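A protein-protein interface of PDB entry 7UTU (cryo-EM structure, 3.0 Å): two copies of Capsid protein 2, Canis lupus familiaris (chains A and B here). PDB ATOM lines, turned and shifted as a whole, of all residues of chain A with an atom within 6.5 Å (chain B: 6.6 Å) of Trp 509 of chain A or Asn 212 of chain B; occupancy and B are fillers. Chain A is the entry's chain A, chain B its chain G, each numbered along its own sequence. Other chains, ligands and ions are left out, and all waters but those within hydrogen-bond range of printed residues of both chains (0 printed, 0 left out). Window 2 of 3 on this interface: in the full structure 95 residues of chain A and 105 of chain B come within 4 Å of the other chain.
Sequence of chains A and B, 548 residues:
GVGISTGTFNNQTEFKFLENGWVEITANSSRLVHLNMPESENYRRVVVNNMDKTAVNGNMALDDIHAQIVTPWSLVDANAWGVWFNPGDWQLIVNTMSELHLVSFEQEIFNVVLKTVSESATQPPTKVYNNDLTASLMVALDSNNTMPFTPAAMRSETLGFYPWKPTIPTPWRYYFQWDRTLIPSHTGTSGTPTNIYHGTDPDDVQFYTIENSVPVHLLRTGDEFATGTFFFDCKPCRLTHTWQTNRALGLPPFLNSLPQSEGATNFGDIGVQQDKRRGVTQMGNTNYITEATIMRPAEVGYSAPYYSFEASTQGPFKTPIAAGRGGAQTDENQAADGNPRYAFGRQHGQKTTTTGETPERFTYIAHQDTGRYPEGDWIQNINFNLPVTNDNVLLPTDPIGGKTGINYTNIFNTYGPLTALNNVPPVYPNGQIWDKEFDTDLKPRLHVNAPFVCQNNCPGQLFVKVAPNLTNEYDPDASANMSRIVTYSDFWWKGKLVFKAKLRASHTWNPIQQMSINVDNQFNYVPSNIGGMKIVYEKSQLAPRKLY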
ATOM      1  N   HIS A 507      12.560 -27.339 -13.056  1.00  0.00           N
ATOM      2  CA  HIS A 507      12.567 -26.030 -12.420  1.00  0.00           C
ATOM      3  C   HIS A 507      13.124 -26.068 -11.008  1.00  0.00           C
ATOM      4  O   HIS A 507      13.768 -25.105 -10.578  1.00  0.00           O
ATOM      5  CB  HIS A 507      11.148 -25.463 -12.379  1.00  0.00           C
ATOM      6  CG  HIS A 507      10.586 -25.146 -13.726  1.00  0.00           C
ATOM      7  ND1 HIS A 507      11.307 -24.484 -14.697  1.00  0.00           N
ATOM      8  CD2 HIS A 507       9.373 -25.403 -14.268  1.00  0.00           C
ATOM      9  CE1 HIS A 507      10.560 -24.345 -15.777  1.00  0.00           C
ATOM     10  NE2 HIS A 507       9.382 -24.894 -15.543  1.00  0.00           N
ATOM     11  N   THR A 508      12.892 -27.155 -10.282  1.00  0.00           N
ATOM     12  CA  THR A 508      13.252 -27.224  -8.879  1.00  0.00           C
ATOM     13  C   THR A 508      14.708 -27.633  -8.701  1.00  0.00           C
ATOM     14  O   THR A 508      15.357 -28.160  -9.608  1.00  0.00           O
ATOM     15  CB  THR A 508      12.357 -28.218  -8.141  1.00  0.00           C
ATOM     16  OG1 THR A 508      12.378 -29.483  -8.817  1.00  0.00           O
ATOM     17  CG2 THR A 508      10.937 -27.708  -8.069  1.00  0.00           C
ATOM     18  N   TRP A 509      15.218 -27.369  -7.499  1.00  0.00           N
ATOM     19  CA  TRP A 509      16.502 -27.923  -7.095  1.00  0.00           C
ATOM     20  C   TRP A 509      16.433 -29.441  -7.003  1.00  0.00           C
ATOM     21  O   TRP A 509      17.369 -30.138  -7.410  1.00  0.00           O
ATOM     22  CB  TRP A 509      16.914 -27.319  -5.752  1.00  0.00           C
ATOM     23  CG  TRP A 509      18.086 -27.976  -5.089  1.00  0.00           C
ATOM     24  CD1 TRP A 509      18.058 -28.981  -4.163  1.00  0.00           C
ATOM     25  CD2 TRP A 509      19.463 -27.652  -5.283  1.00  0.00           C
ATOM     26  NE1 TRP A 509      19.334 -29.309  -3.784  1.00  0.00           N
ATOM     27  CE2 TRP A 509      20.214 -28.504  -4.456  1.00  0.00           C
ATOM     28  CE3 TRP A 509      20.133 -26.723  -6.080  1.00  0.00           C
ATOM     29  CZ2 TRP A 509      21.601 -28.456  -4.405  1.00  0.00           C
ATOM     30  CZ3 TRP A 509      21.507 -26.679  -6.029  1.00  0.00           C
ATOM     31  CH2 TRP A 509      22.228 -27.538  -5.198  1.00  0.00           C
ATOM     32  N   ASN A 510      15.330 -29.965  -6.479  1.00  0.00           N
ATOM     33  CA  ASN A 510      15.266 -31.369  -6.101  1.00  0.00           C
ATOM     34  C   ASN A 510      14.867 -32.243  -7.290  1.00  0.00           C
ATOM     35  O   ASN A 510      14.330 -31.739  -8.280  1.00  0.00           O
ATOM     36  CB  ASN A 510      14.284 -31.575  -4.942  1.00  0.00           C
ATOM     37  CG  ASN A 510      12.881 -31.040  -5.223  1.00  0.00           C
ATOM     38  OD1 ASN A 510      12.483 -30.818  -6.366  1.00  0.00           O
ATOM     39  ND2 ASN A 510      12.138 -30.797  -4.158  1.00  0.00           N
ATOM     40  N   PRO A 511      15.109 -33.554  -7.222  1.00  0.00           N
ATOM     41  CA  PRO A 511      14.591 -34.444  -8.261  1.00  0.00           C
ATOM     42  C   PRO A 511      13.147 -34.842  -7.996  1.00  0.00           C
ATOM     43  O   PRO A 511      12.698 -34.950  -6.852  1.00  0.00           O
ATOM     44  CB  PRO A 511      15.521 -35.656  -8.183  1.00  0.00           C
ATOM     45  CG  PRO A 511      15.931 -35.706  -6.787  1.00  0.00           C
ATOM     46  CD  PRO A 511      15.987 -34.288  -6.293  1.00  0.00           C
ATOM     47  N   TYR B  43      18.758 -20.986   2.789  1.00  0.00           N
ATOM     48  CA  TYR B  43      17.351 -21.359   2.811  1.00  0.00           C
ATOM     49  C   TYR B  43      17.090 -22.312   3.968  1.00  0.00           C
ATOM     50  O   TYR B  43      17.865 -23.244   4.198  1.00  0.00           O
ATOM     51  CB  TYR B  43      16.937 -22.020   1.497  1.00  0.00           C
ATOM     52  CG  TYR B  43      17.178 -21.200   0.250  1.00  0.00           C
ATOM     53  CD1 TYR B  43      16.142 -20.495  -0.339  1.00  0.00           C
ATOM     54  CD2 TYR B  43      18.420 -21.169  -0.364  1.00  0.00           C
ATOM     55  CE1 TYR B  43      16.342 -19.756  -1.481  1.00  0.00           C
ATOM     56  CE2 TYR B  43      18.628 -20.431  -1.507  1.00  0.00           C
ATOM     57  CZ  TYR B  43      17.584 -19.729  -2.061  1.00  0.00           C
ATOM     58  OH  TYR B  43      17.784 -18.995  -3.203  1.00  0.00           O
ATOM     59  N   GLN B 206       8.885 -29.772  -3.483  1.00  0.00           N
ATOM     60  CA  GLN B 206       9.231 -28.730  -4.450  1.00  0.00           C
ATOM     61  C   GLN B 206      10.034 -27.660  -3.718  1.00  0.00           C
ATOM     62  O   GLN B 206       9.465 -26.878  -2.948  1.00  0.00           O
ATOM     63  CB  GLN B 206       7.979 -28.137  -5.085  1.00  0.00           C
ATOM     64  CG  GLN B 206       7.515 -28.818  -6.375  1.00  0.00           C
ATOM     65  CD  GLN B 206       6.504 -28.024  -7.221  1.00  0.00           C
ATOM     66  OE1 GLN B 206       5.991 -27.019  -6.738  1.00  0.00           O
ATOM     67  NE2 GLN B 206       6.243 -28.426  -8.474  1.00  0.00           N
ATOM     68  N   PHE B 207      11.345 -27.620  -3.972  1.00  0.00           N
ATOM     69  CA  PHE B 207      12.253 -26.639  -3.381  1.00  0.00           C
ATOM     70  C   PHE B 207      12.803 -25.766  -4.500  1.00  0.00           C
ATOM     71  O   PHE B 207      13.711 -26.178  -5.225  1.00  0.00           O
ATOM     72  CB  PHE B 207      13.387 -27.333  -2.625  1.00  0.00           C
ATOM     73  CG  PHE B 207      14.479 -26.401  -2.156  1.00  0.00           C
ATOM     74  CD1 PHE B 207      14.180 -25.210  -1.515  1.00  0.00           C
ATOM     75  CD2 PHE B 207      15.808 -26.713  -2.371  1.00  0.00           C
ATOM     76  CE1 PHE B 207      15.181 -24.363  -1.096  1.00  0.00           C
ATOM     77  CE2 PHE B 207      16.810 -25.863  -1.960  1.00  0.00           C
ATOM     78  CZ  PHE B 207      16.496 -24.690  -1.319  1.00  0.00           C
ATOM     79  N   TYR B 208      12.259 -24.560  -4.634  1.00  0.00           N
ATOM     80  CA  TYR B 208      12.724 -23.593  -5.618  1.00  0.00           C
ATOM     81  C   TYR B 208      13.824 -22.732  -5.014  1.00  0.00           C
ATOM     82  O   TYR B 208      13.891 -22.565  -3.793  1.00  0.00           O
ATOM     83  CB  TYR B 208      11.598 -22.689  -6.099  1.00  0.00           C
ATOM     84  CG  TYR B 208      10.337 -23.366  -6.568  1.00  0.00           C
ATOM     85  CD1 TYR B 208      10.152 -23.679  -7.906  1.00  0.00           C
ATOM     86  CD2 TYR B 208       9.301 -23.622  -5.691  1.00  0.00           C
ATOM     87  CE1 TYR B 208       8.978 -24.270  -8.345  1.00  0.00           C
ATOM     88  CE2 TYR B 208       8.128 -24.207  -6.120  1.00  0.00           C
ATOM     89  CZ  TYR B 208       7.971 -24.530  -7.444  1.00  0.00           C
ATOM     90  OH  TYR B 208       6.793 -25.108  -7.857  1.00  0.00           O
ATOM     91  N   THR B 209      14.690 -22.200  -5.875  1.00  0.00           N
ATOM     92  CA  THR B 209      15.718 -21.242  -5.490  1.00  0.00           C
ATOM     93  C   THR B 209      15.777 -20.125  -6.523  1.00  0.00           C
ATOM     94  O   THR B 209      15.588 -20.364  -7.718  1.00  0.00           O
ATOM     95  CB  THR B 209      17.098 -21.898  -5.370  1.00  0.00           C
ATOM     96  OG1 THR B 209      17.540 -22.338  -6.658  1.00  0.00           O
ATOM     97  CG2 THR B 209      17.064 -23.086  -4.417  1.00  0.00           C
ATOM     98  N   ILE B 210      16.045 -18.901  -6.055  1.00  0.00           N
ATOM     99  CA  ILE B 210      16.053 -17.752  -6.958  1.00  0.00           C
ATOM    100  C   ILE B 210      17.238 -17.836  -7.909  1.00  0.00           C
ATOM    101  O   ILE B 210      17.134 -17.459  -9.082  1.00  0.00           O
ATOM    102  CB  ILE B 210      16.045 -16.434  -6.154  1.00  0.00           C
ATOM    103  CG1 ILE B 210      14.608 -16.044  -5.785  1.00  0.00           C
ATOM    104  CG2 ILE B 210      16.724 -15.253  -6.910  1.00  0.00           C
ATOM    105  CD1 ILE B 210      13.806 -15.374  -6.899  1.00  0.00           C
ATOM    106  N   GLU B 211      18.386 -18.307  -7.417  1.00  0.00           N
ATOM    107  CA  GLU B 211      19.599 -18.289  -8.228  1.00  0.00           C
ATOM    108  C   GLU B 211      19.476 -19.218  -9.427  1.00  0.00           C
ATOM    109  O   GLU B 211      19.907 -18.881 -10.535  1.00  0.00           O
ATOM    110  CB  GLU B 211      20.821 -18.668  -7.386  1.00  0.00           C
ATOM    111  CG  GLU B 211      21.158 -17.704  -6.249  1.00  0.00           C
ATOM    112  CD  GLU B 211      20.380 -17.961  -4.976  1.00  0.00           C
ATOM    113  OE1 GLU B 211      19.363 -18.684  -5.029  1.00  0.00           O
ATOM    114  OE2 GLU B 211      20.786 -17.436  -3.919  1.00  0.00           O
ATOM    115  N   ASN B 212      18.886 -20.391  -9.224  1.00  0.00           N
ATOM    116  CA  ASN B 212      18.808 -21.378 -10.286  1.00  0.00           C
ATOM    117  C   ASN B 212      17.718 -21.079 -11.306  1.00  0.00           C
ATOM    118  O   ASN B 212      17.763 -21.631 -12.410  1.00  0.00           O
ATOM    119  CB  ASN B 212      18.565 -22.756  -9.682  1.00  0.00           C
ATOM    120  CG  ASN B 212      19.742 -23.245  -8.867  1.00  0.00           C
ATOM    121  OD1 ASN B 212      20.185 -22.571  -7.943  1.00  0.00           O
ATOM    122  ND2 ASN B 212      20.238 -24.426  -9.188  1.00  0.00           N
ATOM    123  N   SER B 213      16.753 -20.219 -10.974  1.00  0.00           N
ATOM    124  CA  SER B 213      15.540 -20.043 -11.764  1.00  0.00           C
ATOM    125  C   SER B 213      15.552 -18.799 -12.638  1.00  0.00           C
ATOM    126  O   SER B 213      15.180 -18.883 -13.813  1.00  0.00           O
ATOM    127  CB  SER B 213      14.324 -19.981 -10.836  1.00  0.00           C
ATOM    128  OG  SER B 213      14.461 -18.946  -9.880  1.00  0.00           O
ATOM    129  N   VAL B 214      15.982 -17.661 -12.099  1.00  0.00           N
ATOM    130  CA  VAL B 214      15.780 -16.344 -12.707  1.00  0.00           C
ATOM    131  C   VAL B 214      17.163 -15.705 -12.816  1.00  0.00           C
ATOM    132  O   VAL B 214      18.005 -15.963 -11.944  1.00  0.00           O
ATOM    133  CB  VAL B 214      14.793 -15.505 -11.862  1.00  0.00           C
ATOM    134  CG1 VAL B 214      15.139 -15.554 -10.363  1.00  0.00           C
ATOM    135  CG2 VAL B 214      14.627 -14.058 -12.366  1.00  0.00           C
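Gln 206 of chain B touches Thr 508 of chain A (CG to CG2, 3.98 Å).
Thr 508 of chain A touches Phe 207 of chain B (CB to O, 3.8 Å).
CG2 of Thr 508 of chain A touches CE1 of Tyr 208 of chain B, at 3.97 Å.
Trp 509 of chain A touches Asn 212 of chain B (CE3 to ND2, 3.9 Å).
OG1 of Thr 508 of chain A sits at hydrogen-bond distance from OD1 of Asn 510 of chain A (2.8 Å).
The side-chain amide nitrogen (NE2) of Gln 206 of chain B sits close to the side-chain hydroxyl (OH) of Tyr 208 of chain B.
The side-chain hydroxyl of Thr 209 of chain B is in hydrogen-bond range of the side-chain amide oxygen of Asn 212 of chain B (2.9 Å).
The backbone NH of Trp 509 of chain A sits at hydrogen-bond distance from the backbone carbonyl oxygen of Phe 207 of chain B (3.0 Å).
The side-chain amide nitrogen of Asn 510 of chain A lies close to the backbone NH of Gln 206 of chain B, 3.5 Å away.
The side-chain amide nitrogen of Asn 510 of chain A lies close to the backbone NH of Phe 207 of chain B (3.3 Å).
Printed residues of chain A that touch a printed residue of chain B: Thr 508, Trp 509 and Asn 510.
Hydrophobic or aromatic side chains of chain A that line the printed part of chain B: Trp 509.
Among the printed residues, no Asp or Glu carboxylate lies within 4 Å of a Lys or Arg side-chain nitrogen of the other chain.
Asn 212 of chain B touches one residue of chain A.
Of the printed residues of chain A, Tyr 208 of chain B touches Thr 508.
Of the printed residues of chain B, Asn 510 of chain A touches Gln 206 and Phe 207.
Thr 209 of chain B touches none of the printed residues of chain A.
The nearest residue of chain A that does not touch Asn 212 of chain B is His 507 of chain A (5.4 Å).
No position is printed for both chains.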
